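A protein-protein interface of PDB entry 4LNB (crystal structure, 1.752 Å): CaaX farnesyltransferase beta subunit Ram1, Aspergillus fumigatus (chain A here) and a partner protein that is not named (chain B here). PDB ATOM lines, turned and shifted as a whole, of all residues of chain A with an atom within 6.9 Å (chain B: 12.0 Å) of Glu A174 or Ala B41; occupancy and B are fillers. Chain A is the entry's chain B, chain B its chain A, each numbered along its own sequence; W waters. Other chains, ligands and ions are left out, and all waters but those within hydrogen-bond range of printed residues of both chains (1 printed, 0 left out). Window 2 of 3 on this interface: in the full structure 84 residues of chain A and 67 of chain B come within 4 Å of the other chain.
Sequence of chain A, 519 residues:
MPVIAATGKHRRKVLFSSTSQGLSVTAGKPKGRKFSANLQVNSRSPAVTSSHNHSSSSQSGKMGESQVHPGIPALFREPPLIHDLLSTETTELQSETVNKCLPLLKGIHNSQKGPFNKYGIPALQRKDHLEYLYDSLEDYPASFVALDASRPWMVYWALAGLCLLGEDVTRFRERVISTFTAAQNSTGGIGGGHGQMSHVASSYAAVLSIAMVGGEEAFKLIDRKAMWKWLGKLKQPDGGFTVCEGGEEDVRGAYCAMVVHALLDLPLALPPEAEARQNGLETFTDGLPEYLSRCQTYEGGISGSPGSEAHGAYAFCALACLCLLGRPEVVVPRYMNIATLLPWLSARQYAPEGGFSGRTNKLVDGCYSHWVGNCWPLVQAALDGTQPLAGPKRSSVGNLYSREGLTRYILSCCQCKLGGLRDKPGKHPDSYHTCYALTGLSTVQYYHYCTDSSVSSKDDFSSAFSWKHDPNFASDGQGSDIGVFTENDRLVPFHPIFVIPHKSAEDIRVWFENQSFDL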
ATOM      1  N   THR A 170     -35.237  11.686  -5.821  1.00  0.00           N
ATOM      2  CA  THR A 170     -35.278  11.250  -4.429  1.00  0.00           C
ATOM      3  C   THR A 170     -34.121  10.317  -4.075  1.00  0.00           C
ATOM      4  O   THR A 170     -33.760  10.190  -2.909  1.00  0.00           O
ATOM      5  CB  THR A 170     -36.618  10.579  -4.069  1.00  0.00           C
ATOM      6  OG1 THR A 170     -36.898   9.532  -5.005  1.00  0.00           O
ATOM      7  CG2 THR A 170     -37.747  11.599  -4.101  1.00  0.00           C
ATOM      8  N   ARG A 171     -33.528   9.676  -5.077  1.00  0.00           N
ATOM      9  CA  ARG A 171     -32.386   8.803  -4.821  1.00  0.00           C
ATOM     10  C   ARG A 171     -31.135   9.594  -4.432  1.00  0.00           C
ATOM     11  O   ARG A 171     -30.144   9.019  -3.984  1.00  0.00           O
ATOM     12  CB  ARG A 171     -32.100   7.891  -6.019  1.00  0.00           C
ATOM     13  CG  ARG A 171     -31.681   8.610  -7.291  1.00  0.00           C
ATOM     14  CD  ARG A 171     -31.396   7.601  -8.398  1.00  0.00           C
ATOM     15  NE  ARG A 171     -31.069   8.237  -9.671  1.00  0.00           N
ATOM     16  CZ  ARG A 171     -30.833   7.572 -10.798  1.00  0.00           C
ATOM     17  NH1 ARG A 171     -30.887   6.246 -10.810  1.00  0.00           N
ATOM     18  NH2 ARG A 171     -30.544   8.231 -11.912  1.00  0.00           N
ATOM     19  N   PHE A 172     -31.191  10.914  -4.596  1.00  0.00           N
ATOM     20  CA  PHE A 172     -30.076  11.782  -4.215  1.00  0.00           C
ATOM     21  C   PHE A 172     -30.161  12.271  -2.765  1.00  0.00           C
ATOM     22  O   PHE A 172     -29.305  13.034  -2.319  1.00  0.00           O
ATOM     23  CB  PHE A 172     -29.977  12.986  -5.159  1.00  0.00           C
ATOM     24  CG  PHE A 172     -29.342  12.669  -6.482  1.00  0.00           C
ATOM     25  CD1 PHE A 172     -27.974  12.459  -6.574  1.00  0.00           C
ATOM     26  CD2 PHE A 172     -30.107  12.587  -7.633  1.00  0.00           C
ATOM     27  CE1 PHE A 172     -27.383  12.170  -7.791  1.00  0.00           C
ATOM     28  CE2 PHE A 172     -29.522  12.297  -8.853  1.00  0.00           C
ATOM     29  CZ  PHE A 172     -28.159  12.088  -8.932  1.00  0.00           C
ATOM     30  N   ARG A 173     -31.186  11.827  -2.039  1.00  0.00           N
ATOM     31  CA  ARG A 173     -31.422  12.267  -0.660  1.00  0.00           C
ATOM     32  C   ARG A 173     -30.197  12.190   0.250  1.00  0.00           C
ATOM     33  O   ARG A 173     -29.800  13.186   0.852  1.00  0.00           O
ATOM     34  CB  ARG A 173     -32.567  11.475  -0.026  1.00  0.00           C
ATOM     35  CG  ARG A 173     -33.948  11.996  -0.365  1.00  0.00           C
ATOM     36  CD  ARG A 173     -35.029  11.112   0.236  1.00  0.00           C
ATOM     37  NE  ARG A 173     -36.360  11.566  -0.150  1.00  0.00           N
ATOM     38  CZ  ARG A 173     -37.489  10.983   0.233  1.00  0.00           C
ATOM     39  NH1 ARG A 173     -37.452   9.915   1.017  1.00  0.00           N
ATOM     40  NH2 ARG A 173     -38.654  11.469  -0.170  1.00  0.00           N
ATOM     41  N   GLU A 174     -29.604  11.007   0.351  1.00  0.00           N
ATOM     42  CA  GLU A 174     -28.479  10.810   1.261  1.00  0.00           C
ATOM     43  C   GLU A 174     -27.227  11.571   0.824  1.00  0.00           C
ATOM     44  O   GLU A 174     -26.453  12.034   1.664  1.00  0.00           O
ATOM     45  CB  GLU A 174     -28.179   9.319   1.482  1.00  0.00           C
ATOM     46  CG  GLU A 174     -28.614   8.394   0.355  1.00  0.00           C
ATOM     47  CD  GLU A 174     -30.109   8.110   0.358  1.00  0.00           C
ATOM     48  OE1 GLU A 174     -30.758   8.331  -0.687  1.00  0.00           O
ATOM     49  OE2 GLU A 174     -30.631   7.667   1.404  1.00  0.00           O
ATOM     50  N   ARG A 175     -27.032  11.707  -0.484  1.00  0.00           N
ATOM     51  CA  ARG A 175     -25.872  12.440  -0.992  1.00  0.00           C
ATOM     52  C   ARG A 175     -26.029  13.946  -0.790  1.00  0.00           C
ATOM     53  O   ARG A 175     -25.049  14.656  -0.564  1.00  0.00           O
ATOM     54  CB  ARG A 175     -25.608  12.108  -2.462  1.00  0.00           C
ATOM     55  CG  ARG A 175     -25.163  10.667  -2.697  1.00  0.00           C
ATOM     56  CD  ARG A 175     -24.673  10.465  -4.122  1.00  0.00           C
ATOM     57  NE  ARG A 175     -23.369  11.083  -4.344  1.00  0.00           N
ATOM     58  CZ  ARG A 175     -22.782  11.191  -5.531  1.00  0.00           C
ATOM     59  NH1 ARG A 175     -23.389  10.729  -6.617  1.00  0.00           N
ATOM     60  NH2 ARG A 175     -21.593  11.768  -5.637  1.00  0.00           N
ATOM     61  N   VAL A 176     -27.266  14.428  -0.867  1.00  0.00           N
ATOM     62  CA  VAL A 176     -27.561  15.827  -0.566  1.00  0.00           C
ATOM     63  C   VAL A 176     -27.319  16.129   0.914  1.00  0.00           C
ATOM     64  O   VAL A 176     -26.693  17.135   1.260  1.00  0.00           O
ATOM     65  CB  VAL A 176     -29.012  16.187  -0.948  1.00  0.00           C
ATOM     66  CG1 VAL A 176     -29.448  17.478  -0.268  1.00  0.00           C
ATOM     67  CG2 VAL A 176     -29.141  16.303  -2.457  1.00  0.00           C
ATOM     68  N   ILE A 177     -27.811  15.245   1.777  1.00  0.00           N
ATOM     69  CA  ILE A 177     -27.615  15.370   3.219  1.00  0.00           C
ATOM     70  C   ILE A 177     -26.131  15.428   3.565  1.00  0.00           C
ATOM     71  O   ILE A 177     -25.700  16.267   4.359  1.00  0.00           O
ATOM     72  CB  ILE A 177     -28.275  14.197   3.973  1.00  0.00           C
ATOM     73  CG1 ILE A 177     -29.799  14.288   3.869  1.00  0.00           C
ATOM     74  CG2 ILE A 177     -27.836  14.175   5.434  1.00  0.00           C
ATOM     75  CD1 ILE A 177     -30.523  13.055   4.358  1.00  0.00           C
ATOM     76  N   SER A 178     -25.354  14.543   2.952  1.00  0.00           N
ATOM     77  CA  SER A 178     -23.916  14.481   3.183  1.00  0.00           C
ATOM     78  C   SER A 178     -23.222  15.762   2.724  1.00  0.00           C
ATOM     79  O   SER A 178     -22.281  16.237   3.360  1.00  0.00           O
ATOM     80  CB  SER A 178     -23.317  13.274   2.461  1.00  0.00           C
ATOM     81  OG  SER A 178     -21.921  13.187   2.678  1.00  0.00           O
ATOM     82  N   THR A 179     -23.696  16.318   1.614  1.00  0.00           N
ATOM     83  CA  THR A 179     -23.116  17.537   1.061  1.00  0.00           C
ATOM     84  C   THR A 179     -23.348  18.748   1.962  1.00  0.00           C
ATOM     85  O   THR A 179     -22.426  19.511   2.239  1.00  0.00           O
ATOM     86  CB  THR A 179     -23.689  17.840  -0.338  1.00  0.00           C
ATOM     87  OG1 THR A 179     -23.434  16.733  -1.210  1.00  0.00           O
ATOM     88  CG2 THR A 179     -23.056  19.100  -0.918  1.00  0.00           C
ATOM     89  N   VAL A 213     -35.347  16.871  -3.191  1.00  0.00           N
ATOM     90  CA  VAL A 213     -35.129  15.474  -2.819  1.00  0.00           C
ATOM     91  C   VAL A 213     -36.146  15.008  -1.776  1.00  0.00           C
ATOM     92  O   VAL A 213     -36.516  13.834  -1.742  1.00  0.00           O
ATOM     93  CB  VAL A 213     -33.677  15.197  -2.346  1.00  0.00           C
ATOM     94  CG1 VAL A 213     -32.686  15.580  -3.436  1.00  0.00           C
ATOM     95  CG2 VAL A 213     -33.367  15.936  -1.054  1.00  0.00           C
ATOM     96  N   ASN B  34     -13.444  18.789   6.142  1.00  0.00           N
ATOM     97  CA  ASN B  34     -14.524  17.832   6.335  1.00  0.00           C
ATOM     98  C   ASN B  34     -15.469  17.907   5.143  1.00  0.00           C
ATOM     99  O   ASN B  34     -16.438  18.665   5.154  1.00  0.00           O
ATOM    100  CB  ASN B  34     -15.277  18.127   7.634  1.00  0.00           C
ATOM    101  CG  ASN B  34     -16.489  17.231   7.826  1.00  0.00           C
ATOM    102  OD1 ASN B  34     -16.534  16.108   7.323  1.00  0.00           O
ATOM    103  ND2 ASN B  34     -17.481  17.731   8.555  1.00  0.00           N
ATOM    104  N   ASP B  35     -15.182  17.184   4.077  1.00  0.00           N
ATOM    105  CA  ASP B  35     -15.955  17.155   2.809  1.00  0.00           C
ATOM    106  C   ASP B  35     -17.304  16.431   3.042  1.00  0.00           C
ATOM    107  O   ASP B  35     -18.341  16.824   2.552  1.00  0.00           O
ATOM    108  CB  ASP B  35     -15.107  16.368   1.787  1.00  0.00           C
ATOM    109  CG  ASP B  35     -15.414  16.652   0.320  1.00  0.00           C
ATOM    110  OD1 ASP B  35     -15.343  17.774  -0.231  1.00  0.00           O
ATOM    111  OD2 ASP B  35     -15.594  15.648  -0.355  1.00  0.00           O
ATOM    112  N   GLY B  36     -17.262  15.332   3.761  1.00  0.00           N
ATOM    113  CA  GLY B  36     -18.444  14.512   3.937  1.00  0.00           C
ATOM    114  C   GLY B  36     -18.197  13.116   3.404  1.00  0.00           C
ATOM    115  O   GLY B  36     -19.106  12.288   3.343  1.00  0.00           O
ATOM    116  N   SER B  37     -16.950  12.857   3.024  1.00  0.00           N
ATOM    117  CA  SER B  37     -16.554  11.558   2.489  1.00  0.00           C
ATOM    118  C   SER B  37     -16.295  10.550   3.606  1.00  0.00           C
ATOM    119  O   SER B  37     -15.686   9.505   3.382  1.00  0.00           O
ATOM    120  CB  SER B  37     -15.304  11.701   1.620  1.00  0.00           C
ATOM    121  OG  SER B  37     -15.490  12.682   0.614  1.00  0.00           O
ATOM    122  N   ASP B  38     -16.760  10.871   4.810  1.00  0.00           N
ATOM    123  CA  ASP B  38     -16.560  10.013   5.970  1.00  0.00           C
ATOM    124  C   ASP B  38     -17.871   9.768   6.709  1.00  0.00           C
ATOM    125  O   ASP B  38     -18.118   8.669   7.204  1.00  0.00           O
ATOM    126  CB  ASP B  38     -15.542  10.642   6.923  1.00  0.00           C
ATOM    127  CG  ASP B  38     -14.237  10.994   6.236  1.00  0.00           C
ATOM    128  OD1 ASP B  38     -13.785  10.212   5.373  1.00  0.00           O
ATOM    129  OD2 ASP B  38     -13.664  12.058   6.556  1.00  0.00           O
ATOM    130  N   PHE B  39     -18.708  10.800   6.776  1.00  0.00           N
ATOM    131  CA  PHE B  39     -19.968  10.732   7.516  1.00  0.00           C
ATOM    132  C   PHE B  39     -20.943   9.691   6.968  1.00  0.00           C
ATOM    133  O   PHE B  39     -21.750   9.138   7.716  1.00  0.00           O
ATOM    134  CB  PHE B  39     -20.641  12.108   7.570  1.00  0.00           C
ATOM    135  CG  PHE B  39     -20.150  12.982   8.691  1.00  0.00           C
ATOM    136  CD1 PHE B  39     -20.635  12.816   9.978  1.00  0.00           C
ATOM    137  CD2 PHE B  39     -19.212  13.973   8.456  1.00  0.00           C
ATOM    138  CE1 PHE B  39     -20.189  13.618  11.013  1.00  0.00           C
ATOM    139  CE2 PHE B  39     -18.762  14.780   9.487  1.00  0.00           C
ATOM    140  CZ  PHE B  39     -19.252  14.601  10.767  1.00  0.00           C
ATOM    141  N   GLY B  40     -20.872   9.425   5.668  1.00  0.00           N
ATOM    142  CA  GLY B  40     -21.748   8.444   5.054  1.00  0.00           C
ATOM    143  C   GLY B  40     -21.641   8.402   3.542  1.00  0.00           C
ATOM    144  O   GLY B  40     -20.604   8.030   2.993  1.00  0.00           O
ATOM    145  N   ALA B  41     -22.724   8.781   2.869  1.00  0.00           N
ATOM    146  CA  ALA B  41     -22.761   8.791   1.410  1.00  0.00           C
ATOM    147  C   ALA B  41     -21.803   9.832   0.839  1.00  0.00           C
ATOM    148  O   ALA B  41     -21.410  10.770   1.530  1.00  0.00           O
ATOM    149  CB  ALA B  41     -24.178   9.043   0.917  1.00  0.00           C
ATOM    150  N   MET B  42     -21.432   9.659  -0.425  1.00  0.00           N
ATOM    151  CA  MET B  42     -20.496  10.565  -1.080  1.00  0.00           C
ATOM    152  C   MET B  42     -21.158  11.892  -1.437  1.00  0.00           C
ATOM    153  O   MET B  42     -22.238  11.912  -2.022  1.00  0.00           O
ATOM    154  CB  MET B  42     -19.918   9.915  -2.337  1.00  0.00           C
ATOM    155  CG  MET B  42     -18.970   8.759  -2.057  1.00  0.00           C
ATOM    156  SD  MET B  42     -17.491   9.289  -1.171  1.00  0.00           S
ATOM    157  CE  MET B  42     -16.864  10.545  -2.285  1.00  0.00           C
ATOM    158  N   PRO B  43     -20.503  13.010  -1.087  1.00  0.00           N
ATOM    159  CA  PRO B  43     -21.013  14.347  -1.408  1.00  0.00           C
ATOM    160  C   PRO B  43     -21.052  14.601  -2.914  1.00  0.00           C
ATOM    161  O   PRO B  43     -20.449  13.858  -3.693  1.00  0.00           O
ATOM    162  CB  PRO B  43     -20.005  15.282  -0.732  1.00  0.00           C
ATOM    163  CG  PRO B  43     -18.766  14.464  -0.577  1.00  0.00           C
ATOM    164  CD  PRO B  43     -19.235  13.065  -0.339  1.00  0.00           C
ATOM    165  N   LEU B  44     -21.757  15.652  -3.310  1.00  0.00           N
ATOM    166  CA  LEU B  44     -21.968  15.950  -4.719  1.00  0.00           C
ATOM    167  C   LEU B  44     -21.107  17.115  -5.183  1.00  0.00           C
ATOM    168  O   LEU B  44     -20.745  17.981  -4.385  1.00  0.00           O
ATOM    169  CB  LEU B  44     -23.441  16.276  -4.962  1.00  0.00           C
ATOM    170  CG  LEU B  44     -24.410  15.144  -4.625  1.00  0.00           C
ATOM    171  CD1 LEU B  44     -25.797  15.695  -4.337  1.00  0.00           C
ATOM    172  CD2 LEU B  44     -24.452  14.145  -5.766  1.00  0.00           C
ATOM    173  N   ALA B  45     -20.798  17.126  -6.478  1.00  0.00           N
ATOM    174  CA  ALA B  45     -20.054  18.215  -7.113  1.00  0.00           C
ATOM    175  C   ALA B  45     -18.771  18.558  -6.364  1.00  0.00           C
ATOM    176  O   ALA B  45     -18.510  19.718  -6.058  1.00  0.00           O
ATOM    177  CB  ALA B  45     -20.936  19.451  -7.267  1.00  0.00           C
ATOM    178  N   THR B  46     -17.979  17.538  -6.056  1.00  0.00           N
ATOM    179  CA  THR B  46     -16.734  17.752  -5.336  1.00  0.00           C
ATOM    180  C   THR B  46     -15.661  18.316  -6.260  1.00  0.00           C
ATOM    181  O   THR B  46     -15.740  18.184  -7.484  1.00  0.00           O
ATOM    182  CB  THR B  46     -16.229  16.453  -4.679  1.00  0.00           C
ATOM    183  OG1 THR B  46     -16.076  15.436  -5.677  1.00  0.00           O
ATOM    184  CG2 THR B  46     -17.216  15.976  -3.625  1.00  0.00           C
HETATM  185  O   HOH W   1     -19.479  18.677   0.705  1.00  0.00           O
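Val A176 touches just one residue of chain B: Leu B44. Ser A178 touches just these residues of chain B: Gly B36 (3.0 Å) and Ala B41 (2.7 Å). Asp B35 touches none of the printed residues of chain A. Printed residues of chain A within 4 Å of Gly B36: Ser A178. Ala B41 touches just these residues of chain A: Glu A174 (3.8 Å) and Ser A178 (2.7 Å). Of the printed residues of chain A, Met B42 touches Arg A175. Printed residues of chain A within 4 Å of Leu B44: Phe A172 (3.99 Å), Arg A175 (3.4 Å), Val A176 (3.9 Å) and Thr A179 (2.9 Å). The nearest residue of chain B that does not touch Glu A174 is Met B42 (5.6 Å).
Printed residues of chain B that touch a printed residue of chain A: Gly B36, Ala B41, Met B42, Pro B43 and Leu B44. Hydrophobic or aromatic side chains of chain B within 4 Å of the printed part of chain A: Ala B41, Pro B43 and Leu B44. Among the printed residues, no Asp or Glu carboxylate lies within 4 Å of a Lys or Arg side-chain nitrogen of the other chain.
The backbone carbonyl oxygen (O) of Pro B43 is in hydrogen-bond range of the guanidinium group (NH2) of Arg A175, 3.1 Å away. The backbone NH (N) of Leu B44 sits at hydrogen-bond distance from the side-chain hydroxyl (OG1) of Thr A179 (2.9 Å). O of Met B42 sits at hydrogen-bond distance from NE of Arg A175 (2.7 Å). The backbone carbonyl oxygen (O) of Gly B36 lies within hydrogen-bond range of the side-chain hydroxyl (OG) of Ser A178 (3.0 Å). O of Ala B41 sits at hydrogen-bond distance from OG of Ser A178 (2.7 Å).
O of Arg A175 lies within hydrogen-bond range of OG1 of Thr A179 (2.7 Å).
Among the printed residues, pairs that only touch across the chains: Phe A172 with Leu B44 (3.99 Å), Glu A174 with Ala B41 (3.8 Å), Arg A175 with Leu B44 (3.4 Å), Val A176 with Leu B44 (3.9 Å) and Thr A179 with Pro B43 (3.4 Å).
Water W1 lies within hydrogen-bond range of O of Asp B35 (2.9 Å) and O of Thr A179 (3.4 Å).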
